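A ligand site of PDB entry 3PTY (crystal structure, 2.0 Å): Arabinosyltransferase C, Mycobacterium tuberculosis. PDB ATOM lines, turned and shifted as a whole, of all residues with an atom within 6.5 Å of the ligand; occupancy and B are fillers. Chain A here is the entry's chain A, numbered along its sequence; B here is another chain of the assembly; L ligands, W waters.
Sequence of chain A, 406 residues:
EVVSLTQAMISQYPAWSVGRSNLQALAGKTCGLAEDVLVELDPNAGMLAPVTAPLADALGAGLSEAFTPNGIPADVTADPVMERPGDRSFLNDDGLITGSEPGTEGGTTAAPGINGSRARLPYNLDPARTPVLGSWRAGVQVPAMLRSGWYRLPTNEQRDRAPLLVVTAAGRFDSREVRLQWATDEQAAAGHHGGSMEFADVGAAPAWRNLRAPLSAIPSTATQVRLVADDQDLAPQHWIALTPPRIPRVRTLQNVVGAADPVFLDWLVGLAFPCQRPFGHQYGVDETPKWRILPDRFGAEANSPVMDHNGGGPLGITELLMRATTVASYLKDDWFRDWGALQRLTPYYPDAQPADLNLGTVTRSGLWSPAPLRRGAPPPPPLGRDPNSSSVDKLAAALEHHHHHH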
ATOM      1  N   SER A  17      18.791   2.016  -7.861  1.00  0.00           N
ATOM      2  CA  SER A  17      18.713   0.959  -6.855  1.00  0.00           C
ATOM      3  C   SER A  17      18.645  -0.414  -7.521  1.00  0.00           C
ATOM      4  O   SER A  17      19.463  -1.289  -7.219  1.00  0.00           O
ATOM      5  CB  SER A  17      17.519   1.170  -5.923  1.00  0.00           C
ATOM      6  OG  SER A  17      16.291   1.196  -6.637  1.00  0.00           O
ATOM      7  N   VAL A  18      17.677  -0.603  -8.409  1.00  0.00           N
ATOM      8  CA  VAL A  18      17.599  -1.827  -9.195  1.00  0.00           C
ATOM      9  C   VAL A  18      18.816  -1.927 -10.112  1.00  0.00           C
ATOM     10  O   VAL A  18      19.480  -2.959 -10.185  1.00  0.00           O
ATOM     11  CB  VAL A  18      16.323  -1.893 -10.044  1.00  0.00           C
ATOM     12  CG1 VAL A  18      16.326  -3.160 -10.899  1.00  0.00           C
ATOM     13  CG2 VAL A  18      15.096  -1.845  -9.158  1.00  0.00           C
ATOM     14  N   GLY A  19      19.100  -0.832 -10.812  1.00  0.00           N
ATOM     15  CA  GLY A  19      20.257  -0.772 -11.686  1.00  0.00           C
ATOM     16  C   GLY A  19      21.518  -1.133 -10.934  1.00  0.00           C
ATOM     17  O   GLY A  19      22.297  -1.984 -11.365  1.00  0.00           O
ATOM     18  N   ARG A  20      21.705  -0.499  -9.782  1.00  0.00           N
ATOM     19  CA  ARG A  20      22.912  -0.711  -8.989  1.00  0.00           C
ATOM     20  C   ARG A  20      23.049  -2.164  -8.526  1.00  0.00           C
ATOM     21  O   ARG A  20      24.132  -2.737  -8.577  1.00  0.00           O
ATOM     22  CB  ARG A  20      22.946   0.240  -7.792  1.00  0.00           C
ATOM     23  CG  ARG A  20      24.253   0.185  -7.005  1.00  0.00           C
ATOM     24  N   ASN A  22      21.583  -4.918  -9.865  1.00  0.00           N
ATOM     25  CA  ASN A  22      21.848  -5.721 -11.054  1.00  0.00           C
ATOM     26  C   ASN A  22      23.331  -5.753 -11.374  1.00  0.00           C
ATOM     27  O   ASN A  22      23.916  -6.824 -11.568  1.00  0.00           O
ATOM     28  CB  ASN A  22      21.052  -5.207 -12.261  1.00  0.00           C
ATOM     29  CG  ASN A  22      19.575  -5.604 -12.199  1.00  0.00           C
ATOM     30  OD1 ASN A  22      19.159  -6.342 -11.308  1.00  0.00           O
ATOM     31  ND2 ASN A  22      18.795  -5.100 -13.152  1.00  0.00           N
ATOM     32  N   LEU A  23      23.956  -4.576 -11.423  1.00  0.00           N
ATOM     33  CA  LEU A  23      25.367  -4.475 -11.806  1.00  0.00           C
ATOM     34  C   LEU A  23      26.298  -5.091 -10.759  1.00  0.00           C
ATOM     35  O   LEU A  23      27.294  -5.739 -11.101  1.00  0.00           O
ATOM     36  CB  LEU A  23      25.743  -3.019 -12.075  1.00  0.00           C
ATOM     37  CG  LEU A  23      27.171  -2.720 -12.534  1.00  0.00           C
ATOM     38  CD1 LEU A  23      27.550  -3.581 -13.730  1.00  0.00           C
ATOM     39  CD2 LEU A  23      27.351  -1.237 -12.849  1.00  0.00           C
ATOM     40  N   LEU A 331      16.682 -16.794 -18.895  1.00  0.00           N
ATOM     41  CA  LEU A 331      17.420 -16.152 -17.805  1.00  0.00           C
ATOM     42  C   LEU A 331      16.964 -16.705 -16.455  1.00  0.00           C
ATOM     43  O   LEU A 331      15.807 -16.519 -16.072  1.00  0.00           O
ATOM     44  CB  LEU A 331      17.214 -14.645 -17.844  1.00  0.00           C
ATOM     45  CG  LEU A 331      17.975 -13.835 -16.789  1.00  0.00           C
ATOM     46  CD1 LEU A 331      19.484 -14.010 -16.985  1.00  0.00           C
ATOM     47  CD2 LEU A 331      17.583 -12.356 -16.859  1.00  0.00           C
ATOM     48  N   ASP A 333      17.328 -15.744 -13.450  1.00  0.00           N
ATOM     49  CA  ASP A 333      16.832 -14.704 -12.534  1.00  0.00           C
ATOM     50  C   ASP A 333      15.420 -14.198 -12.835  1.00  0.00           C
ATOM     51  O   ASP A 333      14.769 -13.619 -11.969  1.00  0.00           O
ATOM     52  CB  ASP A 333      17.787 -13.511 -12.528  1.00  0.00           C
ATOM     53  CG  ASP A 333      19.213 -13.919 -12.251  1.00  0.00           C
ATOM     54  OD1 ASP A 333      19.963 -14.160 -13.223  1.00  0.00           O
ATOM     55  OD2 ASP A 333      19.572 -14.032 -11.059  1.00  0.00           O
ATOM     56  N   ASP A 334      14.953 -14.392 -14.069  1.00  0.00           N
ATOM     57  CA  ASP A 334      13.628 -13.944 -14.464  1.00  0.00           C
ATOM     58  C   ASP A 334      13.211 -14.702 -15.696  1.00  0.00           C
ATOM     59  O   ASP A 334      13.597 -14.333 -16.795  1.00  0.00           O
ATOM     60  CB  ASP A 334      13.628 -12.432 -14.744  1.00  0.00           C
ATOM     61  CG  ASP A 334      12.238 -11.896 -15.097  1.00  0.00           C
ATOM     62  OD1 ASP A 334      11.284 -12.706 -15.285  1.00  0.00           O
ATOM     63  OD2 ASP A 334      12.114 -10.663 -15.193  1.00  0.00           O
ATOM     64  N   ARG A 337      11.879 -12.839 -18.756  1.00  0.00           N
ATOM     65  CA  ARG A 337      12.658 -11.745 -19.353  1.00  0.00           C
ATOM     66  C   ARG A 337      13.263 -12.146 -20.705  1.00  0.00           C
ATOM     67  O   ARG A 337      13.924 -13.180 -20.810  1.00  0.00           O
ATOM     68  CB  ARG A 337      13.759 -11.304 -18.371  1.00  0.00           C
ATOM     69  CG  ARG A 337      14.866 -10.476 -18.999  1.00  0.00           C
ATOM     70  CD  ARG A 337      14.379  -9.103 -19.380  1.00  0.00           C
ATOM     71  NE  ARG A 337      14.122  -8.302 -18.195  1.00  0.00           N
ATOM     72  CZ  ARG A 337      13.690  -7.049 -18.223  1.00  0.00           C
ATOM     73  NH1 ARG A 337      13.478  -6.442 -19.383  1.00  0.00           N
ATOM     74  NH2 ARG A 337      13.473  -6.402 -17.082  1.00  0.00           N
ATOM     75  N   LEU B 265      16.672   1.487 -24.205  1.00  0.00           N
ATOM     76  CA  LEU B 265      17.843   0.603 -24.348  1.00  0.00           C
ATOM     77  C   LEU B 265      17.553  -0.858 -24.062  1.00  0.00           C
ATOM     78  O   LEU B 265      16.649  -1.190 -23.306  1.00  0.00           O
ATOM     79  CB  LEU B 265      19.041   1.092 -23.526  1.00  0.00           C
ATOM     80  CG  LEU B 265      18.852   1.660 -22.128  1.00  0.00           C
ATOM     81  CD1 LEU B 265      17.901   0.830 -21.328  1.00  0.00           C
ATOM     82  CD2 LEU B 265      20.198   1.784 -21.426  1.00  0.00           C
ATOM     83  N   ASP B 266      18.332  -1.731 -24.712  1.00  0.00           N
ATOM     84  CA  ASP B 266      18.203  -3.178 -24.516  1.00  0.00           C
ATOM     85  C   ASP B 266      18.523  -3.505 -23.054  1.00  0.00           C
ATOM     86  O   ASP B 266      19.372  -2.862 -22.446  1.00  0.00           O
ATOM     87  CB  ASP B 266      19.218  -3.916 -25.392  1.00  0.00           C
ATOM     88  CG  ASP B 266      19.018  -3.663 -26.886  1.00  0.00           C
ATOM     89  OD1 ASP B 266      17.881  -3.822 -27.374  1.00  0.00           O
ATOM     90  OD2 ASP B 266      20.011  -3.321 -27.581  1.00  0.00           O
ATOM     91  N   TRP B 267      17.860  -4.526 -22.515  1.00  0.00           N
ATOM     92  CA  TRP B 267      18.114  -4.935 -21.137  1.00  0.00           C
ATOM     93  C   TRP B 267      19.606  -5.197 -20.882  1.00  0.00           C
ATOM     94  O   TRP B 267      20.164  -4.759 -19.875  1.00  0.00           O
ATOM     95  CB  TRP B 267      17.279  -6.172 -20.783  1.00  0.00           C
ATOM     96  CG  TRP B 267      17.507  -6.654 -19.375  1.00  0.00           C
ATOM     97  CD1 TRP B 267      16.912  -6.183 -18.242  1.00  0.00           C
ATOM     98  CD2 TRP B 267      18.411  -7.692 -18.952  1.00  0.00           C
ATOM     99  NE1 TRP B 267      17.380  -6.867 -17.141  1.00  0.00           N
ATOM    100  CE2 TRP B 267      18.299  -7.793 -17.559  1.00  0.00           C
ATOM    101  CE3 TRP B 267      19.293  -8.537 -19.624  1.00  0.00           C
ATOM    102  CZ2 TRP B 267      19.042  -8.716 -16.813  1.00  0.00           C
ATOM    103  CZ3 TRP B 267      20.020  -9.456 -18.892  1.00  0.00           C
ATOM    104  CH2 TRP B 267      19.893  -9.531 -17.502  1.00  0.00           C
ATOM    105  N   LEU B 268      20.249  -5.916 -21.806  1.00  0.00           N
ATOM    106  CA  LEU B 268      21.674  -6.238 -21.732  1.00  0.00           C
ATOM    107  C   LEU B 268      22.538  -4.987 -21.641  1.00  0.00           C
ATOM    108  O   LEU B 268      23.455  -4.902 -20.811  1.00  0.00           O
ATOM    109  CB  LEU B 268      22.111  -7.027 -22.961  1.00  0.00           C
ATOM    110  CG  LEU B 268      22.292  -8.539 -22.846  1.00  0.00           C
ATOM    111  CD1 LEU B 268      22.817  -9.111 -24.159  1.00  0.00           C
ATOM    112  CD2 LEU B 268      23.229  -8.832 -21.713  1.00  0.00           C
ATOM    113  N   VAL B 269      22.251  -4.031 -22.504  1.00  0.00           N
ATOM    114  CA  VAL B 269      22.990  -2.784 -22.534  1.00  0.00           C
ATOM    115  C   VAL B 269      22.754  -1.961 -21.270  1.00  0.00           C
ATOM    116  O   VAL B 269      23.662  -1.315 -20.763  1.00  0.00           O
ATOM    117  CB  VAL B 269      22.622  -1.945 -23.771  1.00  0.00           C
ATOM    118  CG1 VAL B 269      23.265  -0.551 -23.699  1.00  0.00           C
ATOM    119  CG2 VAL B 269      23.050  -2.681 -25.038  1.00  0.00           C
ATOM    120  N   GLY B 270      21.533  -1.993 -20.748  1.00  0.00           N
ATOM    121  CA  GLY B 270      21.212  -1.243 -19.537  1.00  0.00           C
ATOM    122  C   GLY B 270      22.008  -1.661 -18.305  1.00  0.00           C
ATOM    123  O   GLY B 270      22.110  -0.892 -17.350  1.00  0.00           O
ATOM    124  N   LEU B 271      22.551  -2.867 -18.300  1.00  0.00           N
ATOM    125  CA  LEU B 271      23.317  -3.357 -17.155  1.00  0.00           C
ATOM    126  C   LEU B 271      24.493  -2.430 -16.873  1.00  0.00           C
ATOM    127  O   LEU B 271      24.867  -2.203 -15.718  1.00  0.00           O
ATOM    128  CB  LEU B 271      23.837  -4.773 -17.421  1.00  0.00           C
ATOM    129  CG  LEU B 271      22.785  -5.887 -17.579  1.00  0.00           C
ATOM    130  CD1 LEU B 271      23.473  -7.215 -17.902  1.00  0.00           C
ATOM    131  CD2 LEU B 271      21.954  -6.024 -16.325  1.00  0.00           C
ATOM    132  N   ALA B 272      25.054  -1.871 -17.941  1.00  0.00           N
ATOM    133  CA  ALA B 272      26.211  -0.988 -17.848  1.00  0.00           C
ATOM    134  C   ALA B 272      25.835   0.460 -17.544  1.00  0.00           C
ATOM    135  O   ALA B 272      26.711   1.291 -17.289  1.00  0.00           O
ATOM    136  CB  ALA B 272      27.015  -1.058 -19.153  1.00  0.00           C
ATOM    137  N   PHE B 273      24.533   0.769 -17.563  1.00  0.00           N
ATOM    138  CA  PHE B 273      24.053   2.135 -17.349  1.00  0.00           C
ATOM    139  C   PHE B 273      23.019   2.135 -16.220  1.00  0.00           C
ATOM    140  O   PHE B 273      21.857   2.452 -16.451  1.00  0.00           O
ATOM    141  CB  PHE B 273      23.438   2.701 -18.632  1.00  0.00           C
ATOM    142  CG  PHE B 273      24.440   2.935 -19.738  1.00  0.00           C
ATOM    143  CD1 PHE B 273      24.675   1.953 -20.692  1.00  0.00           C
ATOM    144  CD2 PHE B 273      25.164   4.111 -19.796  1.00  0.00           C
ATOM    145  CE1 PHE B 273      25.607   2.167 -21.704  1.00  0.00           C
ATOM    146  CE2 PHE B 273      26.092   4.327 -20.795  1.00  0.00           C
ATOM    147  CZ  PHE B 273      26.314   3.349 -21.755  1.00  0.00           C
ATOM    148  N   PRO B 274      23.451   1.780 -15.004  1.00  0.00           N
ATOM    149  CA  PRO B 274      22.529   1.563 -13.888  1.00  0.00           C
ATOM    150  C   PRO B 274      21.765   2.819 -13.469  1.00  0.00           C
ATOM    151  O   PRO B 274      20.694   2.681 -12.885  1.00  0.00           O
ATOM    152  CB  PRO B 274      23.472   1.109 -12.763  1.00  0.00           C
ATOM    153  CG  PRO B 274      24.786   1.761 -13.116  1.00  0.00           C
ATOM    154  CD  PRO B 274      24.852   1.561 -14.600  1.00  0.00           C
ATOM    155  N   CYS B 275      22.300   4.001 -13.752  1.00  0.00           N
ATOM    156  CA  CYS B 275      21.648   5.245 -13.305  1.00  0.00           C
ATOM    157  C   CYS B 275      20.676   5.823 -14.337  1.00  0.00           C
ATOM    158  O   CYS B 275      19.963   6.776 -14.049  1.00  0.00           O
ATOM    159  CB  CYS B 275      22.676   6.304 -12.921  1.00  0.00           C
ATOM    160  SG  CYS B 275      23.801   5.859 -11.548  1.00  0.00           S
ATOM    161  N   GLN B 276      20.663   5.264 -15.549  1.00  0.00           N
ATOM    162  CA  GLN B 276      19.734   5.756 -16.570  1.00  0.00           C
ATOM    163  C   GLN B 276      18.360   5.126 -16.397  1.00  0.00           C
ATOM    164  O   GLN B 276      18.237   3.953 -16.073  1.00  0.00           O
ATOM    165  CB  GLN B 276      20.258   5.459 -17.981  1.00  0.00           C
ATOM    166  CG  GLN B 276      21.145   6.566 -18.526  1.00  0.00           C
ATOM    167  CD  GLN B 276      22.349   6.784 -17.651  1.00  0.00           C
ATOM    168  OE1 GLN B 276      23.185   5.889 -17.499  1.00  0.00           O
ATOM    169  NE2 GLN B 276      22.457   7.969 -17.053  1.00  0.00           N
ATOM    170  N   ARG B 277      17.319   5.922 -16.617  1.00  0.00           N
ATOM    171  CA  ARG B 277      15.938   5.469 -16.501  1.00  0.00           C
ATOM    172  C   ARG B 277      15.514   4.740 -17.773  1.00  0.00           C
ATOM    173  O   ARG B 277      15.394   5.349 -18.830  1.00  0.00           O
ATOM    174  CB  ARG B 277      15.017   6.663 -16.256  1.00  0.00           C
ATOM    175  CG  ARG B 277      13.525   6.357 -16.173  1.00  0.00           C
ATOM    176  CD  ARG B 277      12.748   7.683 -16.051  1.00  0.00           C
ATOM    177  NE  ARG B 277      11.291   7.523 -16.087  1.00  0.00           N
ATOM    178  CZ  ARG B 277      10.537   7.356 -14.997  1.00  0.00           C
ATOM    179  NH1 ARG B 277      11.100   7.284 -13.793  1.00  0.00           N
ATOM    180  NH2 ARG B 277       9.223   7.225 -15.125  1.00  0.00           N
ATOM    181  N   PRO B 278      15.257   3.430 -17.669  1.00  0.00           N
ATOM    182  CA  PRO B 278      14.897   2.667 -18.871  1.00  0.00           C
ATOM    183  C   PRO B 278      13.468   2.978 -19.282  1.00  0.00           C
ATOM    184  O   PRO B 278      12.573   2.978 -18.441  1.00  0.00           O
ATOM    185  CB  PRO B 278      15.002   1.202 -18.417  1.00  0.00           C
ATOM    186  CG  PRO B 278      15.669   1.238 -17.069  1.00  0.00           C
ATOM    187  CD  PRO B 278      15.320   2.568 -16.477  1.00  0.00           C
HETATM  188  C1  LIG L   1      17.218  -3.321 -16.359  1.00  0.00           C
HETATM  189  O1  LIG L   1      16.876  -4.414 -15.504  1.00  0.00           O
HETATM  190  C2  LIG L   1      18.713  -3.436 -16.634  1.00  0.00           C
HETATM  191  O2  LIG L   1      19.026  -3.263 -18.024  1.00  0.00           O
HETATM  192  C3  LIG L   1      19.384  -2.375 -15.782  1.00  0.00           C
HETATM  193  O3  LIG L   1      20.276  -3.014 -14.882  1.00  0.00           O
HETATM  194  C4  LIG L   1      18.253  -1.714 -15.000  1.00  0.00           C
HETATM  195  O4  LIG L   1      17.033  -2.085 -15.656  1.00  0.00           O
HETATM  196  C5  LIG L   1      18.404  -0.201 -14.887  1.00  0.00           C
HETATM  197  O5  LIG L   1      17.612   0.267 -13.780  1.00  0.00           O
HETATM  198  C6  LIG L   1      15.516  -4.400 -15.073  1.00  0.00           C
HETATM  199  C7  LIG L   1      15.376  -5.437 -13.964  1.00  0.00           C
HETATM  200  C8  LIG L   1      13.938  -5.908 -13.779  1.00  0.00           C
HETATM  201  C9  LIG L   1      13.843  -6.732 -12.508  1.00  0.00           C
HETATM  202  C10 LIG L   1      15.205  -7.320 -12.123  1.00  0.00           C
HETATM  203  C11 LIG L   1      15.598  -8.512 -12.990  1.00  0.00           C
HETATM  204  C12 LIG L   1      17.045  -8.917 -12.721  1.00  0.00           C
HETATM  205  C13 LIG L   1      17.428 -10.150 -13.498  1.00  0.00           C
HETATM  206  O   HOH W   1      22.540  -1.989 -14.147  1.00  0.00           O
HETATM  207  O   HOH W   2      19.381   1.537 -17.286  1.00  0.00           O
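O of Trp 267 of chain B lies within hydrogen-bond range of O2 of the ligand, 2.6 Å away. O1 of the ligand sits at hydrogen-bond distance from NE1 of Trp 267 of chain B (3.0 Å). The backbone NH (N) of Gly 19 lies within hydrogen-bond range of an oxygen (O5) of the ligand (3.5 Å). An oxygen (O3) of the ligand lies within hydrogen-bond range of the side-chain amide nitrogen (ND2) of Asn 22 (3.1 Å).
Val 18 touches the ligand. Asp 333 touches the ligand (CB to C13, 3.5 Å). NH2 of Arg 337 touches C8 of the ligand, 3.4 Å away. Gly 270 of chain B touches the ligand. Leu 271 of chain B touches the ligand (N to O2, 3.6 Å). Pro 278 of chain B touches the ligand. Hydrophobic or aromatic side chains that line the ligand: Val 18, Trp 267 of chain B, Leu 271 of chain B and Pro 278 of chain B. Within 4 Å of the ligand: Val 18, Gly 19, Asn 22, Asp 333, Arg 337, Trp 267 of chain B, Gly 270 of chain B, Leu 271 of chain B and Pro 278 of chain B. The nearest printed residue that does not touch the ligand is Pro 274 of chain B (4.02 Å).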
